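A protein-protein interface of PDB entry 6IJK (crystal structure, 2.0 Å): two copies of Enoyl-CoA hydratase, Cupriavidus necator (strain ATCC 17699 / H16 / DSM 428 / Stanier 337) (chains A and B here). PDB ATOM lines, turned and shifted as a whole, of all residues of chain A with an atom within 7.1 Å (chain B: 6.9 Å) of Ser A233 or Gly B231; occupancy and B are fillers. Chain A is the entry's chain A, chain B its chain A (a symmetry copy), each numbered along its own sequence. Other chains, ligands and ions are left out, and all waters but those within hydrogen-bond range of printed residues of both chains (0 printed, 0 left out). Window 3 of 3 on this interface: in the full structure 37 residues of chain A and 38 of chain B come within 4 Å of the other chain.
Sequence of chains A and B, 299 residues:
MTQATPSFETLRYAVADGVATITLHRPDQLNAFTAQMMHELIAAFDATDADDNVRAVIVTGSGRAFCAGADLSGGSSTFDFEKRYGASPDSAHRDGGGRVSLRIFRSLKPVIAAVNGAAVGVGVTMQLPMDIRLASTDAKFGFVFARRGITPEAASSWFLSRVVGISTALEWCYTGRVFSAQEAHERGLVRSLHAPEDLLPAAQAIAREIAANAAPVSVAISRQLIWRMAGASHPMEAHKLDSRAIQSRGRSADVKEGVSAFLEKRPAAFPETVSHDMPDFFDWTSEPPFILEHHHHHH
Printed residues of chain B within 4 Å of Ala A230: Arg B162.
Of the printed residues of chain B, Ala A232 touches Trp B158 (3.0 Å) and Arg B162 (3.2 Å).
Ser A233 touches just one residue of chain B: Gly B231 (3.0 Å).
Of the printed residues of chain A, Phe B105 touches His A234 (3.3 Å) and Pro A235 (3.7 Å).
Of the printed residues of chain A, Arg B162 touches Met A229, Ala A230 and Ala A232.
Trp B227 touches none of the printed residues of chain A.
Gly B231 touches just one residue of chain A: Ser A233 (3.0 Å).
Ala B232 touches none of the printed residues of chain A.
The nearest residue of chain B that does not touch Ser A233 is Trp B158 (4.1 Å).
The nearest printed residue of chain B that does not touch Pro A235 is Trp B227 (6.1 Å).
O of Ala A230 lies within hydrogen-bond range of NH2 of Arg B162 (3.0 Å).
O of Ala A232 lies within hydrogen-bond range of NH2 of Arg B162 (3.2 Å).
The backbone carbonyl oxygen (O) of Met A229 is in hydrogen-bond range of the guanidinium group (NH1) of Arg B162 (3.1 Å).
The backbone carbonyl oxygen (O) of Ala A232 lies within hydrogen-bond range of the indole nitrogen (NE1) of Trp B158, 3.0 Å away.
Of the 9 printed residues of chain A, 7 touch a printed residue of chain B.
Of the 13 printed residues of chain B, 5 touch a printed residue of chain A.
Printed residues of chain B that touch a printed residue of chain A: Phe B105, Trp B158, Arg B162, Gly B231 and Pro B288.
Hydrophobic or aromatic side chains of chain B within 4 Å of the printed part of chain A: Phe B105, Trp B158 and Pro B288.
Among the printed residues, no Asp or Glu carboxylate lies within 4 Å of a Lys or Arg side-chain nitrogen of the other chain.
Among the printed residues, merely in contact across the chains: Ser A233 with Gly B231 (3.0 Å), His A234 with Pro B288 (3.3 Å), His A234 with Phe B105 (3.3 Å), Met A236 with Pro B288 (3.3 Å), Met A229 with Trp B158 (3.5 Å), His A234 with Trp B158 (3.6 Å), Pro A235 with Trp B158 (3.7 Å) and Pro A235 with Phe B105 (3.7 Å).
ND1 of His A234 sits at hydrogen-bond distance from N of Met A236 (2.9 Å).
The backbone carbonyl oxygen of Trp B158 is in hydrogen-bond range of the guanidinium group of Arg B162, 2.9 Å away.
Ser A233 touches Gly B231, but with the chains exchanged Gly A231 does not touch Ser B233 (7.5 Å).
Positions printed for both chains: 229, 230, 231, 232, 233 and 234.
Of the 12 pairs that touch across the chains among the printed residues, none has its exchanged pair printed and touching as well.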
ATOM      1  N   MET A 229     -18.250  -3.820 -19.906  1.00  0.00           N
ATOM      2  CA  MET A 229     -18.965  -2.525 -19.824  1.00  0.00           C
ATOM      3  C   MET A 229     -19.025  -2.040 -18.362  1.00  0.00           C
ATOM      4  O   MET A 229     -19.230  -0.809 -18.142  1.00  0.00           O
ATOM      5  CB  MET A 229     -20.355  -2.631 -20.444  1.00  0.00           C
ATOM      6  CG  MET A 229     -20.335  -2.834 -21.963  1.00  0.00           C
ATOM      7  SD  MET A 229     -19.382  -1.512 -22.815  1.00  0.00           S
ATOM      8  CE  MET A 229     -17.856  -2.399 -23.072  1.00  0.00           C
ATOM      9  N   ALA A 230     -18.685  -2.885 -17.390  1.00  0.00           N
ATOM     10  CA  ALA A 230     -18.567  -2.428 -15.986  1.00  0.00           C
ATOM     11  C   ALA A 230     -17.434  -1.379 -15.850  1.00  0.00           C
ATOM     12  O   ALA A 230     -17.522  -0.537 -14.966  1.00  0.00           O
ATOM     13  CB  ALA A 230     -18.379  -3.604 -15.075  1.00  0.00           C
ATOM     14  N   GLY A 231     -16.450  -1.339 -16.744  1.00  0.00           N
ATOM     15  CA  GLY A 231     -15.367  -0.345 -16.708  1.00  0.00           C
ATOM     16  C   GLY A 231     -15.565   0.731 -17.747  1.00  0.00           C
ATOM     17  O   GLY A 231     -14.662   1.563 -17.885  1.00  0.00           O
ATOM     18  N   ALA A 232     -16.688   0.719 -18.480  1.00  0.00           N
ATOM     19  CA  ALA A 232     -16.933   1.703 -19.548  1.00  0.00           C
ATOM     20  C   ALA A 232     -17.424   3.043 -18.950  1.00  0.00           C
ATOM     21  O   ALA A 232     -18.196   3.049 -18.018  1.00  0.00           O
ATOM     22  CB  ALA A 232     -17.872   1.122 -20.555  1.00  0.00           C
ATOM     23  N   SER A 233     -16.985   4.174 -19.494  1.00  0.00           N
ATOM     24  CA  SER A 233     -17.275   5.519 -18.935  1.00  0.00           C
ATOM     25  C   SER A 233     -18.700   5.967 -19.285  1.00  0.00           C
ATOM     26  O   SER A 233     -19.201   6.904 -18.649  1.00  0.00           O
ATOM     27  CB  SER A 233     -16.295   6.548 -19.422  1.00  0.00           C
ATOM     28  OG  SER A 233     -16.528   6.788 -20.802  1.00  0.00           O
ATOM     29  N   HIS A 234     -19.342   5.389 -20.289  1.00  0.00           N
ATOM     30  CA  HIS A 234     -20.679   5.875 -20.706  1.00  0.00           C
ATOM     31  C   HIS A 234     -21.456   4.750 -21.377  1.00  0.00           C
ATOM     32  O   HIS A 234     -20.858   3.941 -22.071  1.00  0.00           O
ATOM     33  CB  HIS A 234     -20.446   7.131 -21.558  1.00  0.00           C
ATOM     34  CG  HIS A 234     -21.678   7.857 -21.948  1.00  0.00           C
ATOM     35  ND1 HIS A 234     -22.578   7.295 -22.817  1.00  0.00           N
ATOM     36  CD2 HIS A 234     -22.128   9.107 -21.632  1.00  0.00           C
ATOM     37  CE1 HIS A 234     -23.550   8.158 -23.010  1.00  0.00           C
ATOM     38  NE2 HIS A 234     -23.304   9.281 -22.293  1.00  0.00           N
ATOM     39  N   PRO A 235     -22.808   4.660 -21.206  1.00  0.00           N
ATOM     40  CA  PRO A 235     -23.616   3.614 -21.856  1.00  0.00           C
ATOM     41  C   PRO A 235     -23.550   3.598 -23.399  1.00  0.00           C
ATOM     42  O   PRO A 235     -23.776   2.538 -23.975  1.00  0.00           O
ATOM     43  CB  PRO A 235     -25.033   3.886 -21.350  1.00  0.00           C
ATOM     44  CG  PRO A 235     -25.015   5.333 -20.955  1.00  0.00           C
ATOM     45  CD  PRO A 235     -23.637   5.548 -20.376  1.00  0.00           C
ATOM     46  N   MET A 236     -23.079   4.674 -24.030  1.00  0.00           N
ATOM     47  CA  MET A 236     -22.858   4.736 -25.497  1.00  0.00           C
ATOM     48  C   MET A 236     -21.957   3.576 -25.903  1.00  0.00           C
ATOM     49  O   MET A 236     -22.258   2.933 -26.962  1.00  0.00           O
ATOM     50  CB  MET A 236     -22.216   6.046 -25.978  1.00  0.00           C
ATOM     51  CG  MET A 236     -22.121   6.143 -27.499  1.00  0.00           C
ATOM     52  SD  MET A 236     -23.698   5.710 -28.382  1.00  0.00           S
ATOM     53  CE  MET A 236     -24.520   7.299 -28.330  1.00  0.00           C
ATOM     54  N   GLU A 237     -20.925   3.279 -25.089  1.00  0.00           N
ATOM     55  CA  GLU A 237     -19.979   2.190 -25.410  1.00  0.00           C
ATOM     56  C   GLU A 237     -20.744   0.875 -25.521  1.00  0.00           C
ATOM     57  O   GLU A 237     -20.471   0.121 -26.470  1.00  0.00           O
ATOM     58  CB  GLU A 237     -18.859   2.071 -24.380  1.00  0.00           C
ATOM     59  CG  GLU A 237     -17.800   3.138 -24.543  1.00  0.00           C
ATOM     60  CD  GLU A 237     -17.163   3.103 -25.919  1.00  0.00           C
ATOM     61  OE1 GLU A 237     -17.169   2.007 -26.550  1.00  0.00           O
ATOM     62  OE2 GLU A 237     -16.698   4.166 -26.379  1.00  0.00           O
ATOM     63  N   PHE B 105     -31.063   8.650 -20.464  1.00  0.00           N
ATOM     64  CA  PHE B 105     -29.782   8.930 -19.782  1.00  0.00           C
ATOM     65  C   PHE B 105     -29.490  10.432 -19.780  1.00  0.00           C
ATOM     66  O   PHE B 105     -29.055  10.929 -18.735  1.00  0.00           O
ATOM     67  CB  PHE B 105     -28.667   8.108 -20.417  1.00  0.00           C
ATOM     68  CG  PHE B 105     -27.338   8.239 -19.724  1.00  0.00           C
ATOM     69  CD1 PHE B 105     -27.067   7.521 -18.571  1.00  0.00           C
ATOM     70  CD2 PHE B 105     -26.365   9.109 -20.204  1.00  0.00           C
ATOM     71  CE1 PHE B 105     -25.833   7.612 -17.952  1.00  0.00           C
ATOM     72  CE2 PHE B 105     -25.151   9.246 -19.538  1.00  0.00           C
ATOM     73  CZ  PHE B 105     -24.881   8.467 -18.445  1.00  0.00           C
ATOM     74  N   TRP B 158     -24.306  -1.994 -19.744  1.00  0.00           N
ATOM     75  CA  TRP B 158     -23.790  -0.878 -18.905  1.00  0.00           C
ATOM     76  C   TRP B 158     -24.669  -0.655 -17.661  1.00  0.00           C
ATOM     77  O   TRP B 158     -24.104  -0.526 -16.588  1.00  0.00           O
ATOM     78  CB  TRP B 158     -23.641   0.421 -19.688  1.00  0.00           C
ATOM     79  CG  TRP B 158     -22.861   1.477 -18.981  1.00  0.00           C
ATOM     80  CD1 TRP B 158     -21.515   1.657 -19.036  1.00  0.00           C
ATOM     81  CD2 TRP B 158     -23.359   2.524 -18.135  1.00  0.00           C
ATOM     82  NE1 TRP B 158     -21.143   2.783 -18.364  1.00  0.00           N
ATOM     83  CE2 TRP B 158     -22.248   3.295 -17.739  1.00  0.00           C
ATOM     84  CE3 TRP B 158     -24.630   2.913 -17.700  1.00  0.00           C
ATOM     85  CZ2 TRP B 158     -22.375   4.421 -16.933  1.00  0.00           C
ATOM     86  CZ3 TRP B 158     -24.743   4.018 -16.891  1.00  0.00           C
ATOM     87  CH2 TRP B 158     -23.638   4.765 -16.525  1.00  0.00           C
ATOM     88  N   ARG B 162     -24.978  -1.606 -12.747  1.00  0.00           N
ATOM     89  CA  ARG B 162     -25.036  -0.419 -11.861  1.00  0.00           C
ATOM     90  C   ARG B 162     -26.369  -0.344 -11.108  1.00  0.00           C
ATOM     91  O   ARG B 162     -26.457   0.452 -10.155  1.00  0.00           O
ATOM     92  CB  ARG B 162     -24.684   0.846 -12.628  1.00  0.00           C
ATOM     93  CG  ARG B 162     -23.231   0.834 -13.077  1.00  0.00           C
ATOM     94  CD  ARG B 162     -23.010   1.726 -14.262  1.00  0.00           C
ATOM     95  NE  ARG B 162     -21.598   1.935 -14.500  1.00  0.00           N
ATOM     96  CZ  ARG B 162     -20.835   1.276 -15.356  1.00  0.00           C
ATOM     97  NH1 ARG B 162     -21.336   0.278 -16.074  1.00  0.00           N
ATOM     98  NH2 ARG B 162     -19.561   1.640 -15.501  1.00  0.00           N
ATOM     99  N   ILE B 226     -24.986  12.748 -11.378  1.00  0.00           N
ATOM    100  CA  ILE B 226     -24.932  11.405 -10.736  1.00  0.00           C
ATOM    101  C   ILE B 226     -24.774  10.331 -11.826  1.00  0.00           C
ATOM    102  O   ILE B 226     -23.912   9.424 -11.682  1.00  0.00           O
ATOM    103  CB  ILE B 226     -26.134  11.184  -9.805  1.00  0.00           C
ATOM    104  CG1 ILE B 226     -25.986  12.053  -8.547  1.00  0.00           C
ATOM    105  CG2 ILE B 226     -26.243   9.699  -9.502  1.00  0.00           C
ATOM    106  CD1 ILE B 226     -27.257  12.156  -7.676  1.00  0.00           C
ATOM    107  N   TRP B 227     -25.538  10.457 -12.911  1.00  0.00           N
ATOM    108  CA  TRP B 227     -25.548   9.435 -13.972  1.00  0.00           C
ATOM    109  C   TRP B 227     -24.183   9.498 -14.702  1.00  0.00           C
ATOM    110  O   TRP B 227     -23.625   8.460 -15.059  1.00  0.00           O
ATOM    111  CB  TRP B 227     -26.744   9.668 -14.904  1.00  0.00           C
ATOM    112  CG  TRP B 227     -28.010   8.957 -14.519  1.00  0.00           C
ATOM    113  CD1 TRP B 227     -29.199   9.505 -14.130  1.00  0.00           C
ATOM    114  CD2 TRP B 227     -28.187   7.535 -14.478  1.00  0.00           C
ATOM    115  NE1 TRP B 227     -30.114   8.513 -13.863  1.00  0.00           N
ATOM    116  CE2 TRP B 227     -29.510   7.292 -14.035  1.00  0.00           C
ATOM    117  CE3 TRP B 227     -27.339   6.442 -14.703  1.00  0.00           C
ATOM    118  CZ2 TRP B 227     -30.018   6.004 -13.902  1.00  0.00           C
ATOM    119  CZ3 TRP B 227     -27.839   5.164 -14.530  1.00  0.00           C
ATOM    120  CH2 TRP B 227     -29.167   4.950 -14.170  1.00  0.00           C
ATOM    121  N   ARG B 228     -23.683  10.693 -14.972  1.00  0.00           N
ATOM    122  CA  ARG B 228     -22.506  10.860 -15.847  1.00  0.00           C
ATOM    123  C   ARG B 228     -21.258  10.523 -15.050  1.00  0.00           C
ATOM    124  O   ARG B 228     -20.428   9.836 -15.600  1.00  0.00           O
ATOM    125  CB  ARG B 228     -22.442  12.258 -16.441  1.00  0.00           C
ATOM    126  CG  ARG B 228     -23.391  12.461 -17.619  1.00  0.00           C
ATOM    127  CD  ARG B 228     -23.290  13.937 -17.948  1.00  0.00           C
ATOM    128  NE  ARG B 228     -24.298  14.324 -18.894  1.00  0.00           N
ATOM    129  CZ  ARG B 228     -24.198  14.218 -20.204  1.00  0.00           C
ATOM    130  NH1 ARG B 228     -23.102  13.717 -20.752  1.00  0.00           N
ATOM    131  NH2 ARG B 228     -25.193  14.637 -20.948  1.00  0.00           N
ATOM    132  N   MET B 229     -21.209  10.890 -13.768  1.00  0.00           N
ATOM    133  CA  MET B 229     -20.008  10.654 -12.932  1.00  0.00           C
ATOM    134  C   MET B 229     -19.932   9.171 -12.514  1.00  0.00           C
ATOM    135  O   MET B 229     -18.812   8.704 -12.150  1.00  0.00           O
ATOM    136  CB  MET B 229     -19.997  11.585 -11.723  1.00  0.00           C
ATOM    137  CG  MET B 229     -19.789  13.058 -12.087  1.00  0.00           C
ATOM    138  SD  MET B 229     -18.254  13.308 -13.069  1.00  0.00           S
ATOM    139  CE  MET B 229     -18.986  13.420 -14.692  1.00  0.00           C
ATOM    140  N   ALA B 230     -20.991   8.390 -12.718  1.00  0.00           N
ATOM    141  CA  ALA B 230     -20.919   6.929 -12.489  1.00  0.00           C
ATOM    142  C   ALA B 230     -19.903   6.277 -13.461  1.00  0.00           C
ATOM    143  O   ALA B 230     -19.329   5.255 -13.106  1.00  0.00           O
ATOM    144  CB  ALA B 230     -22.287   6.323 -12.590  1.00  0.00           C
ATOM    145  N   GLY B 231     -19.592   6.880 -14.605  1.00  0.00           N
ATOM    146  CA  GLY B 231     -18.604   6.347 -15.555  1.00  0.00           C
ATOM    147  C   GLY B 231     -17.299   7.101 -15.482  1.00  0.00           C
ATOM    148  O   GLY B 231     -16.428   6.813 -16.310  1.00  0.00           O
ATOM    149  N   ALA B 232     -17.157   8.051 -14.548  1.00  0.00           N
ATOM    150  CA  ALA B 232     -15.935   8.867 -14.444  1.00  0.00           C
ATOM    151  C   ALA B 232     -14.820   8.083 -13.711  1.00  0.00           C
ATOM    152  O   ALA B 232     -15.089   7.383 -12.761  1.00  0.00           O
ATOM    153  CB  ALA B 232     -16.262  10.176 -13.802  1.00  0.00           C
ATOM    154  N   SER B 233     -13.571   8.210 -14.146  1.00  0.00           N
ATOM    155  CA  SER B 233     -12.433   7.415 -13.616  1.00  0.00           C
ATOM    156  C   SER B 233     -11.961   7.962 -12.263  1.00  0.00           C
ATOM    157  O   SER B 233     -11.245   7.245 -11.550  1.00  0.00           O
ATOM    158  CB  SER B 233     -11.276   7.388 -14.575  1.00  0.00           C
ATOM    159  OG  SER B 233     -10.688   8.680 -14.620  1.00  0.00           O
ATOM    160  N   HIS B 234     -12.275   9.198 -11.909  1.00  0.00           N
ATOM    161  CA  HIS B 234     -11.743   9.779 -10.651  1.00  0.00           C
ATOM    162  C   HIS B 234     -12.677  10.871 -10.146  1.00  0.00           C
ATOM    163  O   HIS B 234     -13.251  11.587 -10.954  1.00  0.00           O
ATOM    164  CB  HIS B 234     -10.299  10.211 -10.940  1.00  0.00           C
ATOM    165  CG  HIS B 234      -9.541  10.682  -9.756  1.00  0.00           C
ATOM    166  ND1 HIS B 234      -9.884  11.847  -9.121  1.00  0.00           N
ATOM    167  CD2 HIS B 234      -8.438  10.176  -9.132  1.00  0.00           C
ATOM    168  CE1 HIS B 234      -9.038  12.038  -8.135  1.00  0.00           C
ATOM    169  NE2 HIS B 234      -8.137  11.026  -8.113  1.00  0.00           N
ATOM    170  N   PRO B 288     -21.557  10.915 -26.243  1.00  0.00           N
ATOM    171  CA  PRO B 288     -20.476  10.486 -27.108  1.00  0.00           C
ATOM    172  C   PRO B 288     -20.999  10.007 -28.472  1.00  0.00           C
ATOM    173  O   PRO B 288     -22.106   9.561 -28.581  1.00  0.00           O
ATOM    174  CB  PRO B 288     -19.921   9.280 -26.355  1.00  0.00           C
ATOM    175  CG  PRO B 288     -20.350   9.487 -24.933  1.00  0.00           C
ATOM    176  CD  PRO B 288     -21.705  10.124 -25.037  1.00  0.00           C
